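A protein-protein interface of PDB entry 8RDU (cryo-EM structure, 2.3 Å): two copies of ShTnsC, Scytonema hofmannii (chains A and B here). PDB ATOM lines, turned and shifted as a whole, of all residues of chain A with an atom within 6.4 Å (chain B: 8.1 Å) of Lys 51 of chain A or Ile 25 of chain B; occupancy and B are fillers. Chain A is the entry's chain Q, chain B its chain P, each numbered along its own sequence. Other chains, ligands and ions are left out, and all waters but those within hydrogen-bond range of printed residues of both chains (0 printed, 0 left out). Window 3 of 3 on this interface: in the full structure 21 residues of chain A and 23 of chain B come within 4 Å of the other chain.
No position is printed for both chains.
Of the 11 printed residues of chain A, 4 touch a printed residue of chain B. Hydrophobic or aromatic side chains of chain A within 4 Å of the printed part of chain B: Ala 52. Of the 20 printed residues of chain B, 5 touch a printed residue of chain A. Along chain B the printed residues that touch a printed residue of chain A span positions 25 to 254. Among the printed residues, 8 pairs touch across the chains. Among the printed residues, Asp or Glu carboxylates within 4 Å of a Lys or Arg side-chain nitrogen of the other chain: Lys 49 of chain A with Glu 250 of chain B and Lys 54 of chain A with Glu 250 of chain B.
Of chain A, only Lys 51 (3.8 Å) comes within 4 Å of Ile 25 of chain B. Printed residues of chain A within 4 Å of Ile 253 of chain B: Lys 51 (3.9 Å) and Ala 52 (3.7 Å). Of the printed residues of chain B, Ala 52 of chain A touches Lys 29 (3.5 Å) and Ile 253 (3.7 Å). Leu 28 of chain B touches none of the printed residues of chain A.
OE2 of Glu 250 of chain B is in salt-bridge range of NH2 of Arg 254 of chain B. O of Ile 253 of chain B lies within hydrogen-bond range of OG of Ser 257 of chain B (2.5 Å). The backbone carbonyl oxygen (O) of Lys 49 of chain A is in hydrogen-bond range of the backbone NH (N) of Lys 54 of chain A, at 3.2 Å.
NZ of Lys 49 of chain A touches NH2 of Arg 254 of chain B (3.8 Å). Lys 51 of chain A touches Ile 25 of chain B. Lys 29 of chain B touches Lys 51 of chain A (CB to O, 3.8 Å). Ile 253 of chain B touches Lys 51 of chain A (CG2 to CD, 3.9 Å). Ala 52 of chain A touches Lys 29 of chain B (O to CB, 3.5 Å). CB of Ala 52 of chain A touches CD1 of Ile 253 of chain B (3.7 Å).
The side-chain carboxylate (OE2) of Glu 250 of chain B lies within salt-bridge range of the side-chain amino group (NZ) of Lys 49 of chain A (2.8 Å). The side-chain amino group (NZ) of Lys 54 of chain A is in salt-bridge range of the side-chain carboxylate (OE1) of Glu 250 of chain B (2.8 Å).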
ATOM      1  N   LEU A  46     -16.972  -0.201  27.108  1.00  0.00           N
ATOM      2  CA  LEU A  46     -16.932   1.217  26.749  1.00  0.00           C
ATOM      3  C   LEU A  46     -16.668   1.454  25.266  1.00  0.00           C
ATOM      4  O   LEU A  46     -17.215   2.394  24.684  1.00  0.00           O
ATOM      5  CB  LEU A  46     -15.880   1.954  27.578  1.00  0.00           C
ATOM      6  CG  LEU A  46     -16.151   2.161  29.061  1.00  0.00           C
ATOM      7  CD1 LEU A  46     -15.049   3.006  29.685  1.00  0.00           C
ATOM      8  CD2 LEU A  46     -17.499   2.823  29.246  1.00  0.00           C
ATOM      9  N   ASP A  47     -15.833   0.634  24.633  1.00  0.00           N
ATOM     10  CA  ASP A  47     -15.703   0.727  23.181  1.00  0.00           C
ATOM     11  C   ASP A  47     -16.996   0.360  22.464  1.00  0.00           C
ATOM     12  O   ASP A  47     -17.385   1.025  21.498  1.00  0.00           O
ATOM     13  CB  ASP A  47     -14.554  -0.153  22.692  1.00  0.00           C
ATOM     14  CG  ASP A  47     -13.201   0.489  22.907  1.00  0.00           C
ATOM     15  OD1 ASP A  47     -13.143   1.735  22.966  1.00  0.00           O
ATOM     16  OD2 ASP A  47     -12.200  -0.246  23.019  1.00  0.00           O
ATOM     17  N   GLY A  48     -17.674  -0.694  22.909  1.00  0.00           N
ATOM     18  CA  GLY A  48     -18.956  -1.027  22.312  1.00  0.00           C
ATOM     19  C   GLY A  48     -20.008   0.043  22.530  1.00  0.00           C
ATOM     20  O   GLY A  48     -20.823   0.314  21.645  1.00  0.00           O
ATOM     21  N   LYS A  49     -20.000   0.666  23.708  1.00  0.00           N
ATOM     22  CA  LYS A  49     -20.981   1.700  24.018  1.00  0.00           C
ATOM     23  C   LYS A  49     -20.684   3.005  23.287  1.00  0.00           C
ATOM     24  O   LYS A  49     -21.596   3.646  22.754  1.00  0.00           O
ATOM     25  CB  LYS A  49     -21.016   1.935  25.525  1.00  0.00           C
ATOM     26  CG  LYS A  49     -22.329   2.470  26.020  1.00  0.00           C
ATOM     27  CD  LYS A  49     -23.381   1.382  26.000  1.00  0.00           C
ATOM     28  CE  LYS A  49     -23.038   0.295  27.008  1.00  0.00           C
ATOM     29  NZ  LYS A  49     -24.033  -0.811  27.017  1.00  0.00           N
ATOM     30  N   ARG A  50     -19.412   3.409  23.252  1.00  0.00           N
ATOM     31  CA  ARG A  50     -18.995   4.561  22.454  1.00  0.00           C
ATOM     32  C   ARG A  50     -19.276   4.353  20.970  1.00  0.00           C
ATOM     33  O   ARG A  50     -19.694   5.285  20.276  1.00  0.00           O
ATOM     34  CB  ARG A  50     -17.515   4.849  22.684  1.00  0.00           C
ATOM     35  CG  ARG A  50     -17.033   6.118  22.020  1.00  0.00           C
ATOM     36  CD  ARG A  50     -15.634   6.480  22.456  1.00  0.00           C
ATOM     37  NE  ARG A  50     -14.676   5.411  22.215  1.00  0.00           N
ATOM     38  CZ  ARG A  50     -13.978   5.279  21.096  1.00  0.00           C
ATOM     39  NH1 ARG A  50     -14.148   6.102  20.076  1.00  0.00           N
ATOM     40  NH2 ARG A  50     -13.083   4.301  21.001  1.00  0.00           N
ATOM     41  N   LYS A  51     -19.033   3.145  20.462  1.00  0.00           N
ATOM     42  CA  LYS A  51     -19.389   2.830  19.082  1.00  0.00           C
ATOM     43  C   LYS A  51     -20.867   3.101  18.816  1.00  0.00           C
ATOM     44  O   LYS A  51     -21.224   3.649  17.767  1.00  0.00           O
ATOM     45  CB  LYS A  51     -19.043   1.371  18.791  1.00  0.00           C
ATOM     46  CG  LYS A  51     -19.306   0.901  17.376  1.00  0.00           C
ATOM     47  CD  LYS A  51     -19.211  -0.613  17.301  1.00  0.00           C
ATOM     48  CE  LYS A  51     -17.868  -1.128  17.804  1.00  0.00           C
ATOM     49  NZ  LYS A  51     -16.735  -0.807  16.893  1.00  0.00           N
ATOM     50  N   ALA A  52     -21.738   2.725  19.748  1.00  0.00           N
ATOM     51  CA  ALA A  52     -23.173   2.948  19.624  1.00  0.00           C
ATOM     52  C   ALA A  52     -23.615   4.317  20.130  1.00  0.00           C
ATOM     53  O   ALA A  52     -24.764   4.704  19.894  1.00  0.00           O
ATOM     54  CB  ALA A  52     -23.943   1.857  20.372  1.00  0.00           C
ATOM     55  N   ARG A  53     -22.730   5.055  20.804  1.00  0.00           N
ATOM     56  CA  ARG A  53     -23.035   6.358  21.407  1.00  0.00           C
ATOM     57  C   ARG A  53     -24.205   6.298  22.387  1.00  0.00           C
ATOM     58  O   ARG A  53     -24.895   7.296  22.603  1.00  0.00           O
ATOM     59  CB  ARG A  53     -23.297   7.419  20.335  1.00  0.00           C
ATOM     60  CG  ARG A  53     -22.164   7.573  19.340  1.00  0.00           C
ATOM     61  CD  ARG A  53     -20.908   8.147  19.993  1.00  0.00           C
ATOM     62  NE  ARG A  53     -19.857   8.404  19.013  1.00  0.00           N
ATOM     63  CZ  ARG A  53     -19.872   9.396  18.136  1.00  0.00           C
ATOM     64  NH1 ARG A  53     -20.797  10.340  18.176  1.00  0.00           N
ATOM     65  NH2 ARG A  53     -18.917   9.463  17.215  1.00  0.00           N
ATOM     66  N   LYS A  54     -24.449   5.130  22.975  1.00  0.00           N
ATOM     67  CA  LYS A  54     -25.401   5.031  24.072  1.00  0.00           C
ATOM     68  C   LYS A  54     -24.817   5.668  25.328  1.00  0.00           C
ATOM     69  O   LYS A  54     -23.605   5.674  25.541  1.00  0.00           O
ATOM     70  CB  LYS A  54     -25.793   3.578  24.328  1.00  0.00           C
ATOM     71  CG  LYS A  54     -27.102   3.188  23.665  1.00  0.00           C
ATOM     72  CD  LYS A  54     -26.961   3.048  22.158  1.00  0.00           C
ATOM     73  CE  LYS A  54     -28.174   2.356  21.551  1.00  0.00           C
ATOM     74  NZ  LYS A  54     -28.342   0.973  22.069  1.00  0.00           N
ATOM     75  N   MET A 140     -17.424  10.376  23.737  1.00  0.00           N
ATOM     76  CA  MET A 140     -17.771   9.832  25.038  1.00  0.00           C
ATOM     77  C   MET A 140     -17.379  10.840  26.107  1.00  0.00           C
ATOM     78  O   MET A 140     -16.328  11.476  26.015  1.00  0.00           O
ATOM     79  CB  MET A 140     -17.076   8.485  25.286  1.00  0.00           C
ATOM     80  CG  MET A 140     -17.218   7.958  26.699  1.00  0.00           C
ATOM     81  SD  MET A 140     -16.784   6.222  26.871  1.00  0.00           S
ATOM     82  CE  MET A 140     -18.201   5.458  26.104  1.00  0.00           C
ATOM     83  N   ALA A 167     -21.899   9.565  24.084  1.00  0.00           N
ATOM     84  CA  ALA A 167     -21.956   8.564  25.150  1.00  0.00           C
ATOM     85  C   ALA A 167     -21.486   9.158  26.474  1.00  0.00           C
ATOM     86  O   ALA A 167     -20.328   9.032  26.878  1.00  0.00           O
ATOM     87  CB  ALA A 167     -21.113   7.353  24.771  1.00  0.00           C
ATOM     88  N   GLU B  19     -16.394  -0.507   3.660  1.00  0.00           N
ATOM     89  CA  GLU B  19     -16.919  -1.779   4.144  1.00  0.00           C
ATOM     90  C   GLU B  19     -18.365  -1.606   4.616  1.00  0.00           C
ATOM     91  O   GLU B  19     -18.769  -0.530   5.053  1.00  0.00           O
ATOM     92  CB  GLU B  19     -16.030  -2.355   5.255  1.00  0.00           C
ATOM     93  CG  GLU B  19     -16.545  -3.659   5.857  1.00  0.00           C
ATOM     94  CD  GLU B  19     -15.576  -4.287   6.834  1.00  0.00           C
ATOM     95  OE1 GLU B  19     -14.961  -3.549   7.628  1.00  0.00           O
ATOM     96  OE2 GLU B  19     -15.438  -5.528   6.809  1.00  0.00           O
ATOM     97  N   TRP B  20     -19.129  -2.695   4.519  1.00  0.00           N
ATOM     98  CA  TRP B  20     -20.560  -2.668   4.799  1.00  0.00           C
ATOM     99  C   TRP B  20     -20.844  -2.401   6.275  1.00  0.00           C
ATOM    100  O   TRP B  20     -21.722  -1.596   6.608  1.00  0.00           O
ATOM    101  CB  TRP B  20     -21.157  -4.010   4.371  1.00  0.00           C
ATOM    102  CG  TRP B  20     -22.642  -4.128   4.415  1.00  0.00           C
ATOM    103  CD1 TRP B  20     -23.393  -4.664   5.418  1.00  0.00           C
ATOM    104  CD2 TRP B  20     -23.555  -3.789   3.365  1.00  0.00           C
ATOM    105  NE1 TRP B  20     -24.723  -4.634   5.079  1.00  0.00           N
ATOM    106  CE2 TRP B  20     -24.850  -4.105   3.821  1.00  0.00           C
ATOM    107  CE3 TRP B  20     -23.407  -3.226   2.093  1.00  0.00           C
ATOM    108  CZ2 TRP B  20     -25.991  -3.878   3.052  1.00  0.00           C
ATOM    109  CZ3 TRP B  20     -24.542  -3.000   1.329  1.00  0.00           C
ATOM    110  CH2 TRP B  20     -25.816  -3.326   1.812  1.00  0.00           C
ATOM    111  N   LEU B  21     -20.111  -3.067   7.172  1.00  0.00           N
ATOM    112  CA  LEU B  21     -20.490  -3.113   8.585  1.00  0.00           C
ATOM    113  C   LEU B  21     -20.460  -1.738   9.253  1.00  0.00           C
ATOM    114  O   LEU B  21     -21.323  -1.427  10.080  1.00  0.00           O
ATOM    115  CB  LEU B  21     -19.576  -4.085   9.328  1.00  0.00           C
ATOM    116  CG  LEU B  21     -19.589  -5.506   8.761  1.00  0.00           C
ATOM    117  CD1 LEU B  21     -18.572  -6.388   9.468  1.00  0.00           C
ATOM    118  CD2 LEU B  21     -20.989  -6.102   8.847  1.00  0.00           C
ATOM    119  N   GLN B  22     -19.471  -0.906   8.913  1.00  0.00           N
ATOM    120  CA  GLN B  22     -19.353   0.425   9.513  1.00  0.00           C
ATOM    121  C   GLN B  22     -20.472   1.374   9.096  1.00  0.00           C
ATOM    122  O   GLN B  22     -20.831   2.273   9.864  1.00  0.00           O
ATOM    123  CB  GLN B  22     -17.994   1.042   9.176  1.00  0.00           C
ATOM    124  CG  GLN B  22     -16.798   0.271   9.703  1.00  0.00           C
ATOM    125  CD  GLN B  22     -16.401  -0.875   8.799  1.00  0.00           C
ATOM    126  OE1 GLN B  22     -17.126  -1.218   7.867  1.00  0.00           O
ATOM    127  NE2 GLN B  22     -15.244  -1.471   9.064  1.00  0.00           N
ATOM    128  N   ALA B  23     -21.022   1.207   7.894  1.00  0.00           N
ATOM    129  CA  ALA B  23     -22.167   2.014   7.483  1.00  0.00           C
ATOM    130  C   ALA B  23     -23.446   1.615   8.208  1.00  0.00           C
ATOM    131  O   ALA B  23     -24.251   2.481   8.573  1.00  0.00           O
ATOM    132  CB  ALA B  23     -22.363   1.913   5.972  1.00  0.00           C
ATOM    133  N   GLU B  24     -23.660   0.318   8.429  1.00  0.00           N
ATOM    134  CA  GLU B  24     -24.776  -0.109   9.270  1.00  0.00           C
ATOM    135  C   GLU B  24     -24.644   0.405  10.698  1.00  0.00           C
ATOM    136  O   GLU B  24     -25.630   0.841  11.299  1.00  0.00           O
ATOM    137  CB  GLU B  24     -24.892  -1.632   9.259  1.00  0.00           C
ATOM    138  CG  GLU B  24     -25.308  -2.197   7.919  1.00  0.00           C
ATOM    139  CD  GLU B  24     -26.588  -1.577   7.399  1.00  0.00           C
ATOM    140  OE1 GLU B  24     -27.607  -1.622   8.118  1.00  0.00           O
ATOM    141  OE2 GLU B  24     -26.572  -1.036   6.277  1.00  0.00           O
ATOM    142  N   ILE B  25     -23.444   0.344  11.272  1.00  0.00           N
ATOM    143  CA  ILE B  25     -23.224   0.945  12.585  1.00  0.00           C
ATOM    144  C   ILE B  25     -23.550   2.435  12.571  1.00  0.00           C
ATOM    145  O   ILE B  25     -24.188   2.954  13.497  1.00  0.00           O
ATOM    146  CB  ILE B  25     -21.781   0.687  13.054  1.00  0.00           C
ATOM    147  CG1 ILE B  25     -21.597  -0.792  13.404  1.00  0.00           C
ATOM    148  CG2 ILE B  25     -21.442   1.563  14.251  1.00  0.00           C
ATOM    149  CD1 ILE B  25     -20.165  -1.254  13.378  1.00  0.00           C
ATOM    150  N   ALA B  26     -23.137   3.144  11.519  1.00  0.00           N
ATOM    151  CA  ALA B  26     -23.402   4.578  11.443  1.00  0.00           C
ATOM    152  C   ALA B  26     -24.890   4.920  11.408  1.00  0.00           C
ATOM    153  O   ALA B  26     -25.288   5.972  11.923  1.00  0.00           O
ATOM    154  CB  ALA B  26     -22.704   5.167  10.218  1.00  0.00           C
ATOM    155  N   ARG B  27     -25.730   4.066  10.817  1.00  0.00           N
ATOM    156  CA  ARG B  27     -27.173   4.257  10.953  1.00  0.00           C
ATOM    157  C   ARG B  27     -27.727   3.727  12.275  1.00  0.00           C
ATOM    158  O   ARG B  27     -28.622   4.346  12.862  1.00  0.00           O
ATOM    159  CB  ARG B  27     -27.904   3.636   9.758  1.00  0.00           C
ATOM    160  CG  ARG B  27     -27.623   2.173   9.511  1.00  0.00           C
ATOM    161  CD  ARG B  27     -28.372   1.654   8.301  1.00  0.00           C
ATOM    162  NE  ARG B  27     -29.800   1.508   8.552  1.00  0.00           N
ATOM    163  CZ  ARG B  27     -30.376   0.368   8.904  1.00  0.00           C
ATOM    164  NH1 ARG B  27     -29.686  -0.756   8.990  1.00  0.00           N
ATOM    165  NH2 ARG B  27     -31.682   0.350   9.149  1.00  0.00           N
ATOM    166  N   LEU B  28     -27.220   2.595  12.763  1.00  0.00           N
ATOM    167  CA  LEU B  28     -27.756   2.026  13.996  1.00  0.00           C
ATOM    168  C   LEU B  28     -27.410   2.854  15.229  1.00  0.00           C
ATOM    169  O   LEU B  28     -28.136   2.796  16.228  1.00  0.00           O
ATOM    170  CB  LEU B  28     -27.270   0.589  14.163  1.00  0.00           C
ATOM    171  CG  LEU B  28     -27.872  -0.408  13.171  1.00  0.00           C
ATOM    172  CD1 LEU B  28     -27.109  -1.728  13.168  1.00  0.00           C
ATOM    173  CD2 LEU B  28     -29.333  -0.631  13.508  1.00  0.00           C
ATOM    174  N   LYS B  29     -26.316   3.610  15.199  1.00  0.00           N
ATOM    175  CA  LYS B  29     -26.060   4.549  16.285  1.00  0.00           C
ATOM    176  C   LYS B  29     -26.886   5.827  16.160  1.00  0.00           C
ATOM    177  O   LYS B  29     -26.852   6.659  17.074  1.00  0.00           O
ATOM    178  CB  LYS B  29     -24.552   4.842  16.401  1.00  0.00           C
ATOM    179  CG  LYS B  29     -23.864   5.623  15.287  1.00  0.00           C
ATOM    180  CD  LYS B  29     -24.021   7.127  15.450  1.00  0.00           C
ATOM    181  CE  LYS B  29     -23.283   7.881  14.360  1.00  0.00           C
ATOM    182  NZ  LYS B  29     -23.559   9.342  14.416  1.00  0.00           N
ATOM    183  N   GLY B  30     -27.606   6.011  15.054  1.00  0.00           N
ATOM    184  CA  GLY B  30     -28.453   7.172  14.875  1.00  0.00           C
ATOM    185  C   GLY B  30     -29.815   7.022  15.534  1.00  0.00           C
ATOM    186  O   GLY B  30     -30.104   6.059  16.245  1.00  0.00           O
ATOM    187  N   ARG B 249     -31.124  -1.712  18.795  1.00  0.00           N
ATOM    188  CA  ARG B 249     -29.913  -1.100  18.256  1.00  0.00           C
ATOM    189  C   ARG B 249     -28.648  -1.586  18.955  1.00  0.00           C
ATOM    190  O   ARG B 249     -27.597  -1.694  18.313  1.00  0.00           O
ATOM    191  CB  ARG B 249     -30.013   0.421  18.341  1.00  0.00           C
ATOM    192  CG  ARG B 249     -31.069   1.025  17.444  1.00  0.00           C
ATOM    193  CD  ARG B 249     -31.156   2.526  17.655  1.00  0.00           C
ATOM    194  NE  ARG B 249     -32.388   3.088  17.119  1.00  0.00           N
ATOM    195  CZ  ARG B 249     -32.477   3.682  15.936  1.00  0.00           C
ATOM    196  NH1 ARG B 249     -31.408   3.879  15.183  1.00  0.00           N
ATOM    197  NH2 ARG B 249     -33.661   4.114  15.512  1.00  0.00           N
ATOM    198  N   GLU B 250     -28.712  -1.866  20.257  1.00  0.00           N
ATOM    199  CA  GLU B 250     -27.564  -2.456  20.939  1.00  0.00           C
ATOM    200  C   GLU B 250     -27.268  -3.854  20.406  1.00  0.00           C
ATOM    201  O   GLU B 250     -26.123  -4.174  20.068  1.00  0.00           O
ATOM    202  CB  GLU B 250     -27.833  -2.502  22.443  1.00  0.00           C
ATOM    203  CG  GLU B 250     -26.616  -2.715  23.332  1.00  0.00           C
ATOM    204  CD  GLU B 250     -25.819  -1.451  23.568  1.00  0.00           C
ATOM    205  OE1 GLU B 250     -26.093  -0.437  22.897  1.00  0.00           O
ATOM    206  OE2 GLU B 250     -24.925  -1.466  24.438  1.00  0.00           O
ATOM    207  N   ALA B 252     -28.312  -5.296  17.523  1.00  0.00           N
ATOM    208  CA  ALA B 252     -27.939  -5.278  16.108  1.00  0.00           C
ATOM    209  C   ALA B 252     -26.501  -4.828  15.879  1.00  0.00           C
ATOM    210  O   ALA B 252     -25.787  -5.428  15.065  1.00  0.00           O
ATOM    211  CB  ALA B 252     -28.900  -4.386  15.324  1.00  0.00           C
ATOM    212  N   ILE B 253     -26.053  -3.780  16.567  1.00  0.00           N
ATOM    213  CA  ILE B 253     -24.657  -3.371  16.435  1.00  0.00           C
ATOM    214  C   ILE B 253     -23.720  -4.477  16.898  1.00  0.00           C
ATOM    215  O   ILE B 253     -22.691  -4.743  16.266  1.00  0.00           O
ATOM    216  CB  ILE B 253     -24.405  -2.056  17.198  1.00  0.00           C
ATOM    217  CG1 ILE B 253     -25.001  -0.878  16.424  1.00  0.00           C
ATOM    218  CG2 ILE B 253     -22.913  -1.852  17.449  1.00  0.00           C
ATOM    219  CD1 ILE B 253     -24.932   0.443  17.144  1.00  0.00           C
ATOM    220  N   ARG B 254     -24.066  -5.152  17.992  1.00  0.00           N
ATOM    221  CA  ARG B 254     -23.266  -6.285  18.448  1.00  0.00           C
ATOM    222  C   ARG B 254     -23.285  -7.439  17.449  1.00  0.00           C
ATOM    223  O   ARG B 254     -22.232  -7.982  17.101  1.00  0.00           O
ATOM    224  CB  ARG B 254     -23.740  -6.738  19.828  1.00  0.00           C
ATOM    225  CG  ARG B 254     -23.351  -5.758  20.915  1.00  0.00           C
ATOM    226  CD  ARG B 254     -23.792  -6.198  22.290  1.00  0.00           C
ATOM    227  NE  ARG B 254     -23.624  -5.118  23.251  1.00  0.00           N
ATOM    228  CZ  ARG B 254     -23.557  -5.282  24.564  1.00  0.00           C
ATOM    229  NH1 ARG B 254     -23.427  -6.483  25.106  1.00  0.00           N
ATOM    230  NH2 ARG B 254     -23.544  -4.211  25.352  1.00  0.00           N
ATOM    231  N   LEU B 256     -23.902  -7.331  14.169  1.00  0.00           N
ATOM    232  CA  LEU B 256     -23.139  -6.970  12.979  1.00  0.00           C
ATOM    233  C   LEU B 256     -21.657  -6.771  13.278  1.00  0.00           C
ATOM    234  O   LEU B 256     -20.824  -6.927  12.378  1.00  0.00           O
ATOM    235  CB  LEU B 256     -23.725  -5.714  12.337  1.00  0.00           C
ATOM    236  CG  LEU B 256     -25.173  -5.874  11.861  1.00  0.00           C
ATOM    237  CD1 LEU B 256     -25.672  -4.612  11.177  1.00  0.00           C
ATOM    238  CD2 LEU B 256     -25.316  -7.087  10.954  1.00  0.00           C
ATOM    239  N   SER B 257     -21.305  -6.432  14.520  1.00  0.00           N
ATOM    240  CA  SER B 257     -19.895  -6.409  14.908  1.00  0.00           C
ATOM    241  C   SER B 257     -19.330  -7.817  15.043  1.00  0.00           C
ATOM    242  O   SER B 257     -18.160  -8.056  14.723  1.00  0.00           O
ATOM    243  CB  SER B 257     -19.716  -5.634  16.211  1.00  0.00           C
ATOM    244  OG  SER B 257     -20.188  -4.305  16.079  1.00  0.00           O
ATOM    245  N   ARG B 258     -20.146  -8.759  15.511  1.00  0.00           N
ATOM    246  CA  ARG B 258     -19.720 -10.137  15.722  1.00  0.00           C
ATOM    247  C   ARG B 258     -19.807 -10.981  14.460  1.00  0.00           C
ATOM    248  O   ARG B 258     -19.391 -12.144  14.483  1.00  0.00           O
ATOM    249  CB  ARG B 258     -20.545 -10.785  16.836  1.00  0.00           C
ATOM    250  CG  ARG B 258     -20.276 -10.199  18.211  1.00  0.00           C
ATOM    251  CD  ARG B 258     -21.189 -10.790  19.268  1.00  0.00           C
ATOM    252  NE  ARG B 258     -20.975 -10.157  20.564  1.00  0.00           N
ATOM    253  CZ  ARG B 258     -21.647 -10.455  21.667  1.00  0.00           C
ATOM    254  NH1 ARG B 258     -22.515 -11.452  21.700  1.00  0.00           N
ATOM    255  NH2 ARG B 258     -21.423  -9.749  22.773  1.00  0.00           N
